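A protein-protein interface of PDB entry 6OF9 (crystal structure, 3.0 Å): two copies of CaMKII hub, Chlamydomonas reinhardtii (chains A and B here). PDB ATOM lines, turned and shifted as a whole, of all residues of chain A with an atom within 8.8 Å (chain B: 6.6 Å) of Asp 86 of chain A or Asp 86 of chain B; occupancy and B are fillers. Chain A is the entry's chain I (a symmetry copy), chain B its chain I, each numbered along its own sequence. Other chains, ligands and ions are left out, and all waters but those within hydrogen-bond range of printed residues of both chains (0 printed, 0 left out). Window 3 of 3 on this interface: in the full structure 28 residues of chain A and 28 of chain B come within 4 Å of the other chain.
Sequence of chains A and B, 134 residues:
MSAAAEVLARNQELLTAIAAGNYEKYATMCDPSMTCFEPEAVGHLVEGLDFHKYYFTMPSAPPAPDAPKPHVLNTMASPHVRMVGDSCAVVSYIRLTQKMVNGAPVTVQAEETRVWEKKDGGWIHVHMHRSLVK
O of Ser 87 of chain B is in hydrogen-bond range of N of Lys 118 of chain B. O of Ser 87 of chain A is in hydrogen-bond range of N of Lys 118 of chain A (2.7 Å).
OD1 of Asp 86 of chain A sits close to OD1 of Asp 86 of chain B, 3.0 Å away.
Of the 8 printed residues of chain B, 5 touch a printed residue of chain A. Printed residues of chain B that touch a printed residue of chain A: Val 84, Gly 85, Asp 86, Ser 87 and Cys 88. Hydrophobic or aromatic side chains of chain B that line the printed part of chain A: Val 84. Of the 14 printed residues of chain A, 6 touch a printed residue of chain B. Among the printed residues, 8 pairs touch across the chains. Among the printed residues, no Asp or Glu carboxylate lies within 4 Å of a Lys or Arg side-chain nitrogen of the other chain.
Asp 86 of chain A touches just one residue of chain B: Asp 86. Asp 86 of chain B touches just one residue of chain A: Asp 86 (3.0 Å). Of chain A, only Ser 87 (3.4 Å) and Glu 117 (3.9 Å) come within 4 Å of Gly 85 of chain B. Printed residues of chain B within 4 Å of Ser 87 of chain A: Gly 85. Of the printed residues of chain A, Cys 88 of chain B touches Val 84 (3.5 Å) and Cys 88 (3.9 Å). Of the printed residues of chain B, Gly 85 of chain A touches Ser 87. Printed residues of chain B within 4 Å of Glu 117 of chain A: Val 84 (3.9 Å) and Gly 85 (3.9 Å). Of the printed residues of chain A, Val 84 of chain B touches Cys 88 (3.5 Å) and Glu 117 (3.9 Å). Met 83 of chain B touches none of the printed residues of chain A. Met 83 of chain A touches none of the printed residues of chain B. The nearest residue of chain A that does not touch Asp 86 of chain B is Ser 87 of chain A (4.9 Å). The nearest printed residue of chain A that does not touch Cys 88 of chain B is Gly 85 of chain A (5.5 Å).
Val 84 of chain A touches Cys 88 of chain B, and with the chains exchanged Cys 88 of chain A touches Val 84 of chain B. Gly 85 of chain A touches Ser 87 of chain B, and with the chains exchanged Ser 87 of chain A touches Gly 85 of chain B. Asp 86 of chain B touches its own counterpart, Asp 86 of chain A. Cys 88 of chain A touches its own counterpart, Cys 88 of chain B. 8 positions are printed for both chains.
Val 84 of chain A touches Cys 88 of chain B (CG2 to SG, 3.5 Å). Ser 87 of chain B touches Gly 85 of chain A (OG to CA, 3.4 Å). Gly 85 of chain B touches Ser 87 of chain A (CA to OG, 3.4 Å). Cys 88 of chain A touches Val 84 of chain B (SG to CG2, 3.5 Å). Cys 88 of chain A touches Cys 88 of chain B. CG1 of Val 84 of chain B touches CD of Glu 117 of chain A, 3.9 Å away. Glu 117 of chain A touches Gly 85 of chain B.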
ATOM      1  N   ALA A   3      -2.866 -12.267  -7.765  1.00  0.00           N
ATOM      2  CA  ALA A   3      -4.239 -12.749  -7.659  1.00  0.00           C
ATOM      3  C   ALA A   3      -5.203 -11.613  -7.333  1.00  0.00           C
ATOM      4  O   ALA A   3      -6.289 -11.527  -7.918  1.00  0.00           O
ATOM      5  CB  ALA A   3      -4.326 -13.850  -6.601  1.00  0.00           C
ATOM      6  N   VAL A   7      -8.415  -9.250  -9.782  1.00  0.00           N
ATOM      7  CA  VAL A   7      -9.788  -9.105  -9.308  1.00  0.00           C
ATOM      8  C   VAL A   7     -10.143  -7.634  -9.123  1.00  0.00           C
ATOM      9  O   VAL A   7     -11.262  -7.208  -9.433  1.00  0.00           O
ATOM     10  CB  VAL A   7      -9.983  -9.902  -8.004  1.00  0.00           C
ATOM     11  CG1 VAL A   7     -11.347  -9.627  -7.410  1.00  0.00           C
ATOM     12  CG2 VAL A   7      -9.807 -11.387  -8.263  1.00  0.00           C
ATOM     13  N   MET A  83      -8.906 -13.693  -0.202  1.00  0.00           N
ATOM     14  CA  MET A  83      -8.920 -14.945  -0.947  1.00  0.00           C
ATOM     15  C   MET A  83      -9.409 -16.056  -0.026  1.00  0.00           C
ATOM     16  O   MET A  83      -8.752 -16.380   0.970  1.00  0.00           O
ATOM     17  CB  MET A  83      -7.534 -15.271  -1.500  1.00  0.00           C
ATOM     18  CG  MET A  83      -6.969 -14.217  -2.442  1.00  0.00           C
ATOM     19  SD  MET A  83      -7.994 -13.918  -3.897  1.00  0.00           S
ATOM     20  CE  MET A  83      -8.110 -15.568  -4.586  1.00  0.00           C
ATOM     21  N   VAL A  84     -10.562 -16.626  -0.353  1.00  0.00           N
ATOM     22  CA  VAL A  84     -11.157 -17.716   0.417  1.00  0.00           C
ATOM     23  C   VAL A  84     -11.190 -18.926  -0.507  1.00  0.00           C
ATOM     24  O   VAL A  84     -12.125 -19.118  -1.290  1.00  0.00           O
ATOM     25  CB  VAL A  84     -12.549 -17.368   0.945  1.00  0.00           C
ATOM     26  CG1 VAL A  84     -12.439 -16.697   2.300  1.00  0.00           C
ATOM     27  CG2 VAL A  84     -13.262 -16.455  -0.037  1.00  0.00           C
ATOM     28  N   GLY A  85     -10.164 -19.758  -0.420  1.00  0.00           N
ATOM     29  CA  GLY A  85     -10.034 -20.861  -1.338  1.00  0.00           C
ATOM     30  C   GLY A  85      -9.355 -20.436  -2.626  1.00  0.00           C
ATOM     31  O   GLY A  85      -8.921 -19.293  -2.801  1.00  0.00           O
ATOM     32  N   ASP A  86      -9.275 -21.391  -3.553  1.00  0.00           N
ATOM     33  CA  ASP A  86      -8.588 -21.151  -4.816  1.00  0.00           C
ATOM     34  C   ASP A  86      -9.386 -20.264  -5.766  1.00  0.00           C
ATOM     35  O   ASP A  86      -8.790 -19.510  -6.543  1.00  0.00           O
ATOM     36  CB  ASP A  86      -8.273 -22.486  -5.502  1.00  0.00           C
ATOM     37  CG  ASP A  86      -9.476 -23.416  -5.559  1.00  0.00           C
ATOM     38  OD1 ASP A  86     -10.176 -23.548  -4.532  1.00  0.00           O
ATOM     39  OD2 ASP A  86      -9.724 -24.015  -6.629  1.00  0.00           O
ATOM     40  N   SER A  87     -10.719 -20.327  -5.719  1.00  0.00           N
ATOM     41  CA  SER A  87     -11.551 -19.785  -6.789  1.00  0.00           C
ATOM     42  C   SER A  87     -12.509 -18.691  -6.328  1.00  0.00           C
ATOM     43  O   SER A  87     -13.453 -18.364  -7.054  1.00  0.00           O
ATOM     44  CB  SER A  87     -12.338 -20.915  -7.458  1.00  0.00           C
ATOM     45  OG  SER A  87     -13.124 -21.616  -6.508  1.00  0.00           O
ATOM     46  N   CYS A  88     -12.297 -18.108  -5.150  1.00  0.00           N
ATOM     47  CA  CYS A  88     -13.197 -17.078  -4.648  1.00  0.00           C
ATOM     48  C   CYS A  88     -12.415 -15.881  -4.127  1.00  0.00           C
ATOM     49  O   CYS A  88     -11.371 -16.034  -3.487  1.00  0.00           O
ATOM     50  CB  CYS A  88     -14.099 -17.617  -3.537  1.00  0.00           C
ATOM     51  SG  CYS A  88     -15.338 -16.421  -2.985  1.00  0.00           S
ATOM     52  N   ALA A  89     -12.945 -14.687  -4.397  1.00  0.00           N
ATOM     53  CA  ALA A  89     -12.348 -13.438  -3.940  1.00  0.00           C
ATOM     54  C   ALA A  89     -13.442 -12.493  -3.464  1.00  0.00           C
ATOM     55  O   ALA A  89     -14.428 -12.267  -4.171  1.00  0.00           O
ATOM     56  CB  ALA A  89     -11.528 -12.779  -5.054  1.00  0.00           C
ATOM     57  N   TRP A 116     -16.519 -12.512  -6.156  1.00  0.00           N
ATOM     58  CA  TRP A 116     -16.145 -12.964  -7.485  1.00  0.00           C
ATOM     59  C   TRP A 116     -15.679 -14.410  -7.405  1.00  0.00           C
ATOM     60  O   TRP A 116     -15.019 -14.809  -6.440  1.00  0.00           O
ATOM     61  CB  TRP A 116     -15.042 -12.080  -8.075  1.00  0.00           C
ATOM     62  CG  TRP A 116     -15.436 -10.639  -8.209  1.00  0.00           C
ATOM     63  CD1 TRP A 116     -15.461  -9.699  -7.219  1.00  0.00           C
ATOM     64  CD2 TRP A 116     -15.859  -9.973  -9.405  1.00  0.00           C
ATOM     65  NE1 TRP A 116     -15.877  -8.490  -7.724  1.00  0.00           N
ATOM     66  CE2 TRP A 116     -16.128  -8.632  -9.064  1.00  0.00           C
ATOM     67  CE3 TRP A 116     -16.040 -10.381 -10.729  1.00  0.00           C
ATOM     68  CZ2 TRP A 116     -16.565  -7.698 -10.001  1.00  0.00           C
ATOM     69  CZ3 TRP A 116     -16.473  -9.452 -11.658  1.00  0.00           C
ATOM     70  CH2 TRP A 116     -16.731  -8.127 -11.290  1.00  0.00           C
ATOM     71  N   GLU A 117     -16.034 -15.190  -8.423  1.00  0.00           N
ATOM     72  CA  GLU A 117     -15.690 -16.601  -8.505  1.00  0.00           C
ATOM     73  C   GLU A 117     -14.889 -16.848  -9.775  1.00  0.00           C
ATOM     74  O   GLU A 117     -15.191 -16.276 -10.829  1.00  0.00           O
ATOM     75  CB  GLU A 117     -16.954 -17.474  -8.500  1.00  0.00           C
ATOM     76  CG  GLU A 117     -16.695 -18.975  -8.540  1.00  0.00           C
ATOM     77  CD  GLU A 117     -17.978 -19.786  -8.586  1.00  0.00           C
ATOM     78  OE1 GLU A 117     -19.030 -19.218  -8.946  1.00  0.00           O
ATOM     79  OE2 GLU A 117     -17.934 -20.990  -8.258  1.00  0.00           O
ATOM     80  N   LYS A 118     -13.859 -17.689  -9.673  1.00  0.00           N
ATOM     81  CA  LYS A 118     -13.071 -18.058 -10.849  1.00  0.00           C
ATOM     82  C   LYS A 118     -13.809 -19.177 -11.575  1.00  0.00           C
ATOM     83  O   LYS A 118     -13.636 -20.364 -11.294  1.00  0.00           O
ATOM     84  CB  LYS A 118     -11.654 -18.467 -10.467  1.00  0.00           C
ATOM     85  CG  LYS A 118     -10.755 -18.681 -11.681  1.00  0.00           C
ATOM     86  CD  LYS A 118      -9.360 -19.160 -11.304  1.00  0.00           C
ATOM     87  CE  LYS A 118      -8.509 -18.039 -10.739  1.00  0.00           C
ATOM     88  NZ  LYS A 118      -7.085 -18.459 -10.597  1.00  0.00           N
ATOM     89  N   LYS A 119     -14.645 -18.775 -12.526  1.00  0.00           N
ATOM     90  CA  LYS A 119     -15.436 -19.672 -13.353  1.00  0.00           C
ATOM     91  C   LYS A 119     -15.040 -19.475 -14.810  1.00  0.00           C
ATOM     92  O   LYS A 119     -14.780 -18.345 -15.243  1.00  0.00           O
ATOM     93  CB  LYS A 119     -16.938 -19.404 -13.153  1.00  0.00           C
ATOM     94  CG  LYS A 119     -17.874 -20.142 -14.101  1.00  0.00           C
ATOM     95  CD  LYS A 119     -19.326 -19.742 -13.855  1.00  0.00           C
ATOM     96  CE  LYS A 119     -19.927 -20.480 -12.665  1.00  0.00           C
ATOM     97  NZ  LYS A 119     -20.312 -21.877 -13.017  1.00  0.00           N
ATOM     98  N   TRP A 123     -12.971 -14.317 -13.973  1.00  0.00           N
ATOM     99  CA  TRP A 123     -13.625 -13.878 -12.747  1.00  0.00           C
ATOM    100  C   TRP A 123     -15.032 -13.392 -13.077  1.00  0.00           C
ATOM    101  O   TRP A 123     -15.205 -12.498 -13.913  1.00  0.00           O
ATOM    102  CB  TRP A 123     -12.816 -12.780 -12.051  1.00  0.00           C
ATOM    103  CG  TRP A 123     -11.553 -13.293 -11.425  1.00  0.00           C
ATOM    104  CD1 TRP A 123     -10.290 -13.199 -11.935  1.00  0.00           C
ATOM    105  CD2 TRP A 123     -11.430 -13.992 -10.178  1.00  0.00           C
ATOM    106  NE1 TRP A 123      -9.389 -13.791 -11.081  1.00  0.00           N
ATOM    107  CE2 TRP A 123     -10.064 -14.287  -9.997  1.00  0.00           C
ATOM    108  CE3 TRP A 123     -12.342 -14.394  -9.195  1.00  0.00           C
ATOM    109  CZ2 TRP A 123      -9.586 -14.963  -8.874  1.00  0.00           C
ATOM    110  CZ3 TRP A 123     -11.865 -15.069  -8.081  1.00  0.00           C
ATOM    111  CH2 TRP A 123     -10.501 -15.346  -7.931  1.00  0.00           C
ATOM    112  N   MET B  83     -22.312 -21.584  -2.671  1.00  0.00           N
ATOM    113  CA  MET B  83     -21.030 -22.272  -2.617  1.00  0.00           C
ATOM    114  C   MET B  83     -20.150 -21.757  -3.750  1.00  0.00           C
ATOM    115  O   MET B  83     -20.471 -21.947  -4.929  1.00  0.00           O
ATOM    116  CB  MET B  83     -21.212 -23.786  -2.718  1.00  0.00           C
ATOM    117  CG  MET B  83     -22.071 -24.390  -1.617  1.00  0.00           C
ATOM    118  SD  MET B  83     -21.426 -24.107   0.045  1.00  0.00           S
ATOM    119  CE  MET B  83     -19.780 -24.798  -0.099  1.00  0.00           C
ATOM    120  N   VAL B  84     -19.055 -21.100  -3.392  1.00  0.00           N
ATOM    121  CA  VAL B  84     -18.101 -20.559  -4.358  1.00  0.00           C
ATOM    122  C   VAL B  84     -16.790 -21.301  -4.128  1.00  0.00           C
ATOM    123  O   VAL B  84     -15.974 -20.928  -3.280  1.00  0.00           O
ATOM    124  CB  VAL B  84     -17.926 -19.046  -4.223  1.00  0.00           C
ATOM    125  CG1 VAL B  84     -18.946 -18.326  -5.083  1.00  0.00           C
ATOM    126  CG2 VAL B  84     -18.079 -18.634  -2.770  1.00  0.00           C
ATOM    127  N   GLY B  85     -16.577 -22.363  -4.889  1.00  0.00           N
ATOM    128  CA  GLY B  85     -15.432 -23.210  -4.665  1.00  0.00           C
ATOM    129  C   GLY B  85     -15.710 -24.248  -3.595  1.00  0.00           C
ATOM    130  O   GLY B  85     -16.815 -24.366  -3.055  1.00  0.00           O
ATOM    131  N   ASP B  86     -14.664 -25.013  -3.280  1.00  0.00           N
ATOM    132  CA  ASP B  86     -14.797 -26.102  -2.319  1.00  0.00           C
ATOM    133  C   ASP B  86     -14.900 -25.611  -0.878  1.00  0.00           C
ATOM    134  O   ASP B  86     -15.570 -26.251  -0.061  1.00  0.00           O
ATOM    135  CB  ASP B  86     -13.610 -27.063  -2.450  1.00  0.00           C
ATOM    136  CG  ASP B  86     -12.269 -26.343  -2.468  1.00  0.00           C
ATOM    137  OD1 ASP B  86     -12.151 -25.322  -3.178  1.00  0.00           O
ATOM    138  OD2 ASP B  86     -11.333 -26.796  -1.773  1.00  0.00           O
ATOM    139  N   SER B  87     -14.262 -24.485  -0.547  1.00  0.00           N
ATOM    140  CA  SER B  87     -14.024 -24.119   0.845  1.00  0.00           C
ATOM    141  C   SER B  87     -14.653 -22.789   1.247  1.00  0.00           C
ATOM    142  O   SER B  87     -14.286 -22.233   2.288  1.00  0.00           O
ATOM    143  CB  SER B  87     -12.519 -24.087   1.123  1.00  0.00           C
ATOM    144  OG  SER B  87     -11.860 -23.191   0.243  1.00  0.00           O
ATOM    145  N   CYS B  88     -15.591 -22.261   0.465  1.00  0.00           N
ATOM    146  CA  CYS B  88     -16.204 -20.978   0.785  1.00  0.00           C
ATOM    147  C   CYS B  88     -17.718 -21.055   0.664  1.00  0.00           C
ATOM    148  O   CYS B  88     -18.251 -21.684  -0.255  1.00  0.00           O
ATOM    149  CB  CYS B  88     -15.677 -19.865  -0.121  1.00  0.00           C
ATOM    150  SG  CYS B  88     -16.293 -18.227   0.336  1.00  0.00           S
ATOM    151  N   LYS B 118     -13.887 -22.896   4.911  1.00  0.00           N
ATOM    152  CA  LYS B 118     -13.578 -24.204   5.490  1.00  0.00           C
ATOM    153  C   LYS B 118     -12.087 -24.236   5.806  1.00  0.00           C
ATOM    154  O   LYS B 118     -11.251 -24.593   4.976  1.00  0.00           O
ATOM    155  CB  LYS B 118     -13.986 -25.339   4.559  1.00  0.00           C
ATOM    156  CG  LYS B 118     -13.846 -26.713   5.208  1.00  0.00           C
ATOM    157  CD  LYS B 118     -14.182 -27.851   4.255  1.00  0.00           C
ATOM    158  CE  LYS B 118     -15.678 -27.988   4.040  1.00  0.00           C
ATOM    159  NZ  LYS B 118     -16.007 -29.241   3.303  1.00  0.00           N
ATOM    160  N   TRP B 123     -15.836 -24.646   9.788  1.00  0.00           N
ATOM    161  CA  TRP B 123     -16.279 -23.408   9.158  1.00  0.00           C
ATOM    162  C   TRP B 123     -15.957 -22.237  10.078  1.00  0.00           C
ATOM    163  O   TRP B 123     -16.381 -22.217  11.239  1.00  0.00           O
ATOM    164  CB  TRP B 123     -17.775 -23.456   8.836  1.00  0.00           C
ATOM    165  CG  TRP B 123     -18.099 -24.380   7.699  1.00  0.00           C
ATOM    166  CD1 TRP B 123     -18.593 -25.649   7.791  1.00  0.00           C
ATOM    167  CD2 TRP B 123     -17.939 -24.112   6.298  1.00  0.00           C
ATOM    168  NE1 TRP B 123     -18.755 -26.186   6.535  1.00  0.00           N
ATOM    169  CE2 TRP B 123     -18.359 -25.264   5.602  1.00  0.00           C
ATOM    170  CE3 TRP B 123     -17.485 -23.010   5.565  1.00  0.00           C
ATOM    171  CZ2 TRP B 123     -18.341 -25.345   4.209  1.00  0.00           C
ATOM    172  CZ3 TRP B 123     -17.465 -23.095   4.180  1.00  0.00           C
ATOM    173  CH2 TRP B 123     -17.890 -24.254   3.519  1.00  0.00           C
